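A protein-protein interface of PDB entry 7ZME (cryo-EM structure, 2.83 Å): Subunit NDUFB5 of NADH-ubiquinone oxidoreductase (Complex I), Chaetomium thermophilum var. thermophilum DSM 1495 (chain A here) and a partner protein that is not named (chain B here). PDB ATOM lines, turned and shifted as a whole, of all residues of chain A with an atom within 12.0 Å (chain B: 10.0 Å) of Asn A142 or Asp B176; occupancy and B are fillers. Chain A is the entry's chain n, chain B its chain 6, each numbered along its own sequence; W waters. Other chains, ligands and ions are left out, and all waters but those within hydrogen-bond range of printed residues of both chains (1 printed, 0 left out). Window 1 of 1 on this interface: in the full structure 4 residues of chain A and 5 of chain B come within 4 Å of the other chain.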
ATOM      1  N   GLY A 138     -10.427 -29.609 -21.832  1.00  0.00           N
ATOM      2  CA  GLY A 138      -9.267 -28.959 -21.200  1.00  0.00           C
ATOM      3  C   GLY A 138      -7.977 -29.674 -21.524  1.00  0.00           C
ATOM      4  O   GLY A 138      -8.005 -30.905 -21.591  1.00  0.00           O
ATOM      5  N   SER A 139      -6.880 -28.931 -21.655  1.00  0.00           N
ATOM      6  CA  SER A 139      -5.566 -29.510 -22.049  1.00  0.00           C
ATOM      7  C   SER A 139      -4.956 -30.371 -20.945  1.00  0.00           C
ATOM      8  O   SER A 139      -5.038 -29.976 -19.775  1.00  0.00           O
ATOM      9  CB  SER A 139      -4.613 -28.432 -22.495  1.00  0.00           C
ATOM     10  OG  SER A 139      -3.379 -28.981 -22.922  1.00  0.00           O
ATOM     11  N   PRO A 140      -4.320 -31.516 -21.280  1.00  0.00           N
ATOM     12  CA  PRO A 140      -3.628 -32.347 -20.284  1.00  0.00           C
ATOM     13  C   PRO A 140      -2.164 -31.942 -20.089  1.00  0.00           C
ATOM     14  O   PRO A 140      -1.439 -32.674 -19.471  1.00  0.00           O
ATOM     15  CB  PRO A 140      -3.671 -33.718 -20.952  1.00  0.00           C
ATOM     16  CG  PRO A 140      -3.609 -33.428 -22.426  1.00  0.00           C
ATOM     17  CD  PRO A 140      -4.347 -32.122 -22.608  1.00  0.00           C
ATOM     18  N   PHE A 141      -1.772 -30.769 -20.568  1.00  0.00           N
ATOM     19  CA  PHE A 141      -0.352 -30.360 -20.554  1.00  0.00           C
ATOM     20  C   PHE A 141      -0.158 -28.955 -20.024  1.00  0.00           C
ATOM     21  O   PHE A 141      -1.078 -28.154 -20.175  1.00  0.00           O
ATOM     22  CB  PHE A 141       0.192 -30.287 -21.980  1.00  0.00           C
ATOM     23  CG  PHE A 141      -0.100 -31.476 -22.852  1.00  0.00           C
ATOM     24  CD1 PHE A 141       0.427 -32.718 -22.550  1.00  0.00           C
ATOM     25  CD2 PHE A 141      -0.888 -31.347 -23.981  1.00  0.00           C
ATOM     26  CE1 PHE A 141       0.159 -33.812 -23.353  1.00  0.00           C
ATOM     27  CE2 PHE A 141      -1.158 -32.445 -24.784  1.00  0.00           C
ATOM     28  CZ  PHE A 141      -0.637 -33.674 -24.462  1.00  0.00           C
ATOM     29  N   ASN A 142       0.943 -28.743 -19.300  1.00  0.00           N
ATOM     30  CA  ASN A 142       1.314 -27.395 -18.814  1.00  0.00           C
ATOM     31  C   ASN A 142       0.231 -26.897 -17.880  1.00  0.00           C
ATOM     32  O   ASN A 142      -0.094 -25.710 -17.924  1.00  0.00           O
ATOM     33  CB  ASN A 142       1.643 -26.457 -19.977  1.00  0.00           C
ATOM     34  CG  ASN A 142       2.903 -26.828 -20.721  1.00  0.00           C
ATOM     35  OD1 ASN A 142       3.731 -27.579 -20.213  1.00  0.00           O
ATOM     36  ND2 ASN A 142       3.050 -26.298 -21.922  1.00  0.00           N
ATOM     37  N   VAL A 143      -0.284 -27.791 -17.049  1.00  0.00           N
ATOM     38  CA  VAL A 143      -1.425 -27.416 -16.173  1.00  0.00           C
ATOM     39  C   VAL A 143      -0.880 -26.786 -14.901  1.00  0.00           C
ATOM     40  O   VAL A 143      -0.036 -27.414 -14.247  1.00  0.00           O
ATOM     41  CB  VAL A 143      -2.327 -28.629 -15.878  1.00  0.00           C
ATOM     42  CG1 VAL A 143      -3.502 -28.258 -14.991  1.00  0.00           C
ATOM     43  CG2 VAL A 143      -2.808 -29.300 -17.151  1.00  0.00           C
ATOM     44  N   PRO A 144      -1.305 -25.557 -14.544  1.00  0.00           N
ATOM     45  CA  PRO A 144      -0.915 -24.970 -13.269  1.00  0.00           C
ATOM     46  C   PRO A 144      -1.566 -25.787 -12.147  1.00  0.00           C
ATOM     47  O   PRO A 144      -2.619 -26.331 -12.373  1.00  0.00           O
ATOM     48  CB  PRO A 144      -1.476 -23.544 -13.367  1.00  0.00           C
ATOM     49  CG  PRO A 144      -1.671 -23.307 -14.843  1.00  0.00           C
ATOM     50  CD  PRO A 144      -2.101 -24.654 -15.373  1.00  0.00           C
ATOM     51  N   ALA A 145      -0.917 -25.896 -10.988  1.00  0.00           N
ATOM     52  CA  ALA A 145      -1.546 -26.594  -9.840  1.00  0.00           C
ATOM     53  C   ALA A 145      -2.667 -25.732  -9.273  1.00  0.00           C
ATOM     54  O   ALA A 145      -2.421 -24.542  -9.010  1.00  0.00           O
ATOM     55  CB  ALA A 145      -0.538 -26.911  -8.775  1.00  0.00           C
ATOM     56  N   GLY A 146      -3.842 -26.324  -9.080  1.00  0.00           N
ATOM     57  CA  GLY A 146      -4.999 -25.588  -8.557  1.00  0.00           C
ATOM     58  C   GLY A 146      -5.728 -24.866  -9.658  1.00  0.00           C
ATOM     59  O   GLY A 146      -6.387 -23.865  -9.363  1.00  0.00           O
ATOM     60  N   PHE A 147      -5.581 -25.329 -10.896  1.00  0.00           N
ATOM     61  CA  PHE A 147      -6.215 -24.574 -12.010  1.00  0.00           C
ATOM     62  C   PHE A 147      -7.631 -25.091 -12.303  1.00  0.00           C
ATOM     63  O   PHE A 147      -8.555 -24.274 -12.340  1.00  0.00           O
ATOM     64  CB  PHE A 147      -5.300 -24.611 -13.233  1.00  0.00           C
ATOM     65  CG  PHE A 147      -5.898 -24.081 -14.509  1.00  0.00           C
ATOM     66  CD1 PHE A 147      -5.716 -22.761 -14.880  1.00  0.00           C
ATOM     67  CD2 PHE A 147      -6.632 -24.908 -15.343  1.00  0.00           C
ATOM     68  CE1 PHE A 147      -6.262 -22.278 -16.057  1.00  0.00           C
ATOM     69  CE2 PHE A 147      -7.196 -24.418 -16.507  1.00  0.00           C
ATOM     70  CZ  PHE A 147      -6.998 -23.108 -16.865  1.00  0.00           C
ATOM     71  N   TYR A 148      -7.792 -26.388 -12.509  1.00  0.00           N
ATOM     72  CA  TYR A 148      -9.117 -26.962 -12.832  1.00  0.00           C
ATOM     73  C   TYR A 148     -10.027 -26.911 -11.603  1.00  0.00           C
ATOM     74  O   TYR A 148      -9.586 -27.241 -10.498  1.00  0.00           O
ATOM     75  CB  TYR A 148      -8.944 -28.369 -13.403  1.00  0.00           C
ATOM     76  CG  TYR A 148      -8.424 -28.424 -14.814  1.00  0.00           C
ATOM     77  CD1 TYR A 148      -9.175 -27.936 -15.867  1.00  0.00           C
ATOM     78  CD2 TYR A 148      -7.190 -28.980 -15.099  1.00  0.00           C
ATOM     79  CE1 TYR A 148      -8.709 -27.986 -17.168  1.00  0.00           C
ATOM     80  CE2 TYR A 148      -6.709 -29.039 -16.395  1.00  0.00           C
ATOM     81  CZ  TYR A 148      -7.471 -28.536 -17.432  1.00  0.00           C
ATOM     82  OH  TYR A 148      -7.004 -28.581 -18.710  1.00  0.00           O
ATOM     83  N   LYS B 173       5.442 -14.232 -14.415  1.00  0.00           N
ATOM     84  CA  LYS B 173       5.887 -15.556 -14.920  1.00  0.00           C
ATOM     85  C   LYS B 173       5.253 -16.726 -14.154  1.00  0.00           C
ATOM     86  O   LYS B 173       4.841 -16.508 -13.011  1.00  0.00           O
ATOM     87  CB  LYS B 173       7.413 -15.576 -14.837  1.00  0.00           C
ATOM     88  CG  LYS B 173       8.020 -15.748 -13.455  1.00  0.00           C
ATOM     89  CD  LYS B 173       9.526 -15.808 -13.488  1.00  0.00           C
ATOM     90  CE  LYS B 173      10.152 -14.619 -14.184  1.00  0.00           C
ATOM     91  NZ  LYS B 173      11.629 -14.724 -14.218  1.00  0.00           N
ATOM     92  N   ILE B 174       5.124 -17.905 -14.781  1.00  0.00           N
ATOM     93  CA  ILE B 174       4.665 -19.133 -14.049  1.00  0.00           C
ATOM     94  C   ILE B 174       5.618 -20.278 -14.373  1.00  0.00           C
ATOM     95  O   ILE B 174       6.245 -20.242 -15.430  1.00  0.00           O
ATOM     96  CB  ILE B 174       3.202 -19.572 -14.289  1.00  0.00           C
ATOM     97  CG1 ILE B 174       2.845 -19.684 -15.772  1.00  0.00           C
ATOM     98  CG2 ILE B 174       2.220 -18.706 -13.512  1.00  0.00           C
ATOM     99  CD1 ILE B 174       1.546 -20.412 -16.017  1.00  0.00           C
ATOM    100  N   TRP B 175       5.727 -21.234 -13.463  1.00  0.00           N
ATOM    101  CA  TRP B 175       6.664 -22.365 -13.648  1.00  0.00           C
ATOM    102  C   TRP B 175       5.928 -23.654 -14.021  1.00  0.00           C
ATOM    103  O   TRP B 175       6.449 -24.391 -14.863  1.00  0.00           O
ATOM    104  CB  TRP B 175       7.515 -22.482 -12.382  1.00  0.00           C
ATOM    105  CG  TRP B 175       8.360 -21.264 -12.183  1.00  0.00           C
ATOM    106  CD1 TRP B 175       8.126 -20.233 -11.324  1.00  0.00           C
ATOM    107  CD2 TRP B 175       9.554 -20.920 -12.906  1.00  0.00           C
ATOM    108  NE1 TRP B 175       9.107 -19.288 -11.440  1.00  0.00           N
ATOM    109  CE2 TRP B 175       9.995 -19.679 -12.405  1.00  0.00           C
ATOM    110  CE3 TRP B 175      10.299 -21.542 -13.913  1.00  0.00           C
ATOM    111  CZ2 TRP B 175      11.146 -19.053 -12.877  1.00  0.00           C
ATOM    112  CZ3 TRP B 175      11.436 -20.923 -14.381  1.00  0.00           C
ATOM    113  CH2 TRP B 175      11.852 -19.698 -13.865  1.00  0.00           C
ATOM    114  N   ASP B 176       4.766 -23.902 -13.422  1.00  0.00           N
ATOM    115  CA  ASP B 176       3.948 -25.109 -13.722  1.00  0.00           C
ATOM    116  C   ASP B 176       3.424 -25.079 -15.166  1.00  0.00           C
ATOM    117  O   ASP B 176       3.410 -26.138 -15.810  1.00  0.00           O
ATOM    118  CB  ASP B 176       2.894 -25.357 -12.640  1.00  0.00           C
ATOM    119  CG  ASP B 176       2.230 -24.097 -12.111  1.00  0.00           C
ATOM    120  OD1 ASP B 176       1.565 -24.189 -11.060  1.00  0.00           O
ATOM    121  OD2 ASP B 176       2.361 -23.040 -12.755  1.00  0.00           O
ATOM    122  N   GLY B 177       3.011 -23.914 -15.651  1.00  0.00           N
ATOM    123  CA  GLY B 177       2.497 -23.781 -17.025  1.00  0.00           C
ATOM    124  C   GLY B 177       3.598 -23.567 -18.032  1.00  0.00           C
ATOM    125  O   GLY B 177       3.285 -23.495 -19.222  1.00  0.00           O
ATOM    126  N   ALA B 178       4.842 -23.443 -17.576  1.00  0.00           N
ATOM    127  CA  ALA B 178       5.991 -23.306 -18.497  1.00  0.00           C
ATOM    128  C   ALA B 178       6.830 -24.583 -18.552  1.00  0.00           C
ATOM    129  O   ALA B 178       7.971 -24.481 -19.020  1.00  0.00           O
ATOM    130  CB  ALA B 178       6.842 -22.133 -18.098  1.00  0.00           C
ATOM    131  N   LEU B 179       6.326 -25.724 -18.076  1.00  0.00           N
ATOM    132  CA  LEU B 179       7.220 -26.910 -18.038  1.00  0.00           C
ATOM    133  C   LEU B 179       7.665 -27.299 -19.451  1.00  0.00           C
ATOM    134  O   LEU B 179       8.875 -27.418 -19.663  1.00  0.00           O
ATOM    135  CB  LEU B 179       6.471 -28.071 -17.376  1.00  0.00           C
ATOM    136  CG  LEU B 179       7.156 -29.434 -17.468  1.00  0.00           C
ATOM    137  CD1 LEU B 179       8.325 -29.528 -16.504  1.00  0.00           C
ATOM    138  CD2 LEU B 179       6.170 -30.554 -17.202  1.00  0.00           C
ATOM    139  N   ALA B 180       6.732 -27.449 -20.386  1.00  0.00           N
ATOM    140  CA  ALA B 180       7.082 -27.745 -21.792  1.00  0.00           C
ATOM    141  C   ALA B 180       6.256 -26.852 -22.717  1.00  0.00           C
ATOM    142  O   ALA B 180       5.365 -27.392 -23.369  1.00  0.00           O
ATOM    143  CB  ALA B 180       6.815 -29.193 -22.064  1.00  0.00           C
ATOM    144  N   GLU B 181       6.716 -25.503 -22.790  1.00  0.00           N
ATOM    145  CA  GLU B 181       5.938 -24.580 -23.660  1.00  0.00           C
ATOM    146  C   GLU B 181       5.906 -25.095 -25.094  1.00  0.00           C
ATOM    147  O   GLU B 181       6.959 -25.524 -25.586  1.00  0.00           O
ATOM    148  CB  GLU B 181       6.416 -23.134 -23.587  1.00  0.00           C
ATOM    149  CG  GLU B 181       5.764 -22.193 -24.575  1.00  0.00           C
ATOM    150  CD  GLU B 181       6.772 -21.267 -25.227  1.00  0.00           C
ATOM    151  OE1 GLU B 181       7.970 -21.406 -24.922  1.00  0.00           O
ATOM    152  OE2 GLU B 181       6.360 -20.419 -26.040  1.00  0.00           O
ATOM    153  N   ASN B 182       4.578 -25.065 -25.706  1.00  0.00           N
ATOM    154  CA  ASN B 182       4.533 -25.511 -27.114  1.00  0.00           C
ATOM    155  C   ASN B 182       4.519 -24.274 -27.996  1.00  0.00           C
ATOM    156  O   ASN B 182       4.177 -23.199 -27.491  1.00  0.00           O
ATOM    157  CB  ASN B 182       3.285 -26.346 -27.411  1.00  0.00           C
ATOM    158  CG  ASN B 182       3.212 -27.659 -26.666  1.00  0.00           C
ATOM    159  OD1 ASN B 182       4.100 -27.992 -25.892  1.00  0.00           O
ATOM    160  ND2 ASN B 182       2.154 -28.412 -26.902  1.00  0.00           N
ATOM    161  N   ASN B 183       4.879 -24.428 -29.264  1.00  0.00           N
ATOM    162  CA  ASN B 183       4.738 -23.301 -30.217  1.00  0.00           C
ATOM    163  C   ASN B 183       3.261 -23.299 -30.598  1.00  0.00           C
ATOM    164  O   ASN B 183       2.614 -24.326 -30.387  1.00  0.00           O
ATOM    165  CB  ASN B 183       5.696 -23.424 -31.401  1.00  0.00           C
ATOM    166  CG  ASN B 183       7.150 -23.467 -30.983  1.00  0.00           C
ATOM    167  OD1 ASN B 183       7.926 -24.260 -31.505  1.00  0.00           O
ATOM    168  ND2 ASN B 183       7.521 -22.625 -30.033  1.00  0.00           N
ATOM    169  N   SER B 186       2.142 -26.148 -32.777  1.00  0.00           N
ATOM    170  CA  SER B 186       2.087 -27.413 -32.007  1.00  0.00           C
ATOM    171  C   SER B 186       0.807 -27.470 -31.168  1.00  0.00           C
ATOM    172  O   SER B 186       0.207 -28.539 -31.089  1.00  0.00           O
ATOM    173  CB  SER B 186       3.318 -27.577 -31.183  1.00  0.00           C
ATOM    174  OG  SER B 186       3.501 -28.936 -30.829  1.00  0.00           O
ATOM    175  N   SER B 187       0.406 -26.350 -30.580  1.00  0.00           N
ATOM    176  CA  SER B 187      -0.828 -26.285 -29.762  1.00  0.00           C
ATOM    177  C   SER B 187      -2.051 -26.576 -30.630  1.00  0.00           C
ATOM    178  O   SER B 187      -2.977 -27.238 -30.134  1.00  0.00           O
ATOM    179  CB  SER B 187      -0.938 -24.965 -29.073  1.00  0.00           C
ATOM    180  OG  SER B 187       0.281 -24.635 -28.431  1.00  0.00           O
ATOM    181  N   ASN B 190      -2.025 -30.251 -31.442  1.00  0.00           N
ATOM    182  CA  ASN B 190      -2.448 -31.076 -30.316  1.00  0.00           C
ATOM    183  C   ASN B 190      -3.933 -31.410 -30.365  1.00  0.00           C
ATOM    184  O   ASN B 190      -4.347 -32.427 -29.800  1.00  0.00           O
ATOM    185  CB  ASN B 190      -2.128 -30.370 -28.999  1.00  0.00           C
ATOM    186  CG  ASN B 190      -0.649 -30.403 -28.655  1.00  0.00           C
ATOM    187  OD1 ASN B 190      -0.201 -29.705 -27.748  1.00  0.00           O
ATOM    188  ND2 ASN B 190       0.112 -31.211 -29.376  1.00  0.00           N
HETATM  189  O   HOH W   1       2.479 -28.626 -14.970  1.00  0.00           O
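O of Ala B180 lies close to OD1 of Asn B182, at 2.9 Å.
Among the printed residues, merely in contact across the chains: Asn A142 with Gly B177, Pro A144 with Asp B176, Asn A142 with Glu B181, Asn A142 with Leu B179, Asn A142 with Asp B176 and Val A143 with Asp B176.
O of Ala B180 is in hydrogen-bond range of ND2 of Asn A142 (2.9 Å). N of Ala A145 sits at hydrogen-bond distance from OD1 of Asp B176, 3.0 Å away.
Printed residues of chain B that touch a printed residue of chain A: Asp B176, Gly B177, Leu B179, Ala B180 and Glu B181. Hydrophobic or aromatic side chains of chain B that line the printed part of chain A: Leu B179 and Ala B180. Along chain B the printed residues that touch a printed residue of chain A span positions 176 to 181. Of the 11 printed residues of chain A, 4 touch a printed residue of chain B. Printed residues of chain A that touch a printed residue of chain B: Asn A142, Val A143, Pro A144 and Ala A145. Hydrophobic or aromatic side chains of chain A that line the printed part of chain B: Pro A144. Among the printed residues, no Asp or Glu carboxylate lies within 4 Å of a Lys or Arg side-chain nitrogen of the other chain.
Water W1 bridges O of Asp B176 and O of Val A143.
Asn A142 touches just these residues of chain B: Asp B176, Gly B177, Leu B179, Ala B180 and Glu B181. No residue of chain A comes within 4 Å of Ile B174. Of the printed residues of chain A, Gly B177 touches Asn A142 (3.4 Å). Ala B178 touches none of the printed residues of chain A. Leu B179 touches just one residue of chain A: Asn A142 (3.8 Å). Printed residues of chain A within 4 Å of Ala B180: Asn A142.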
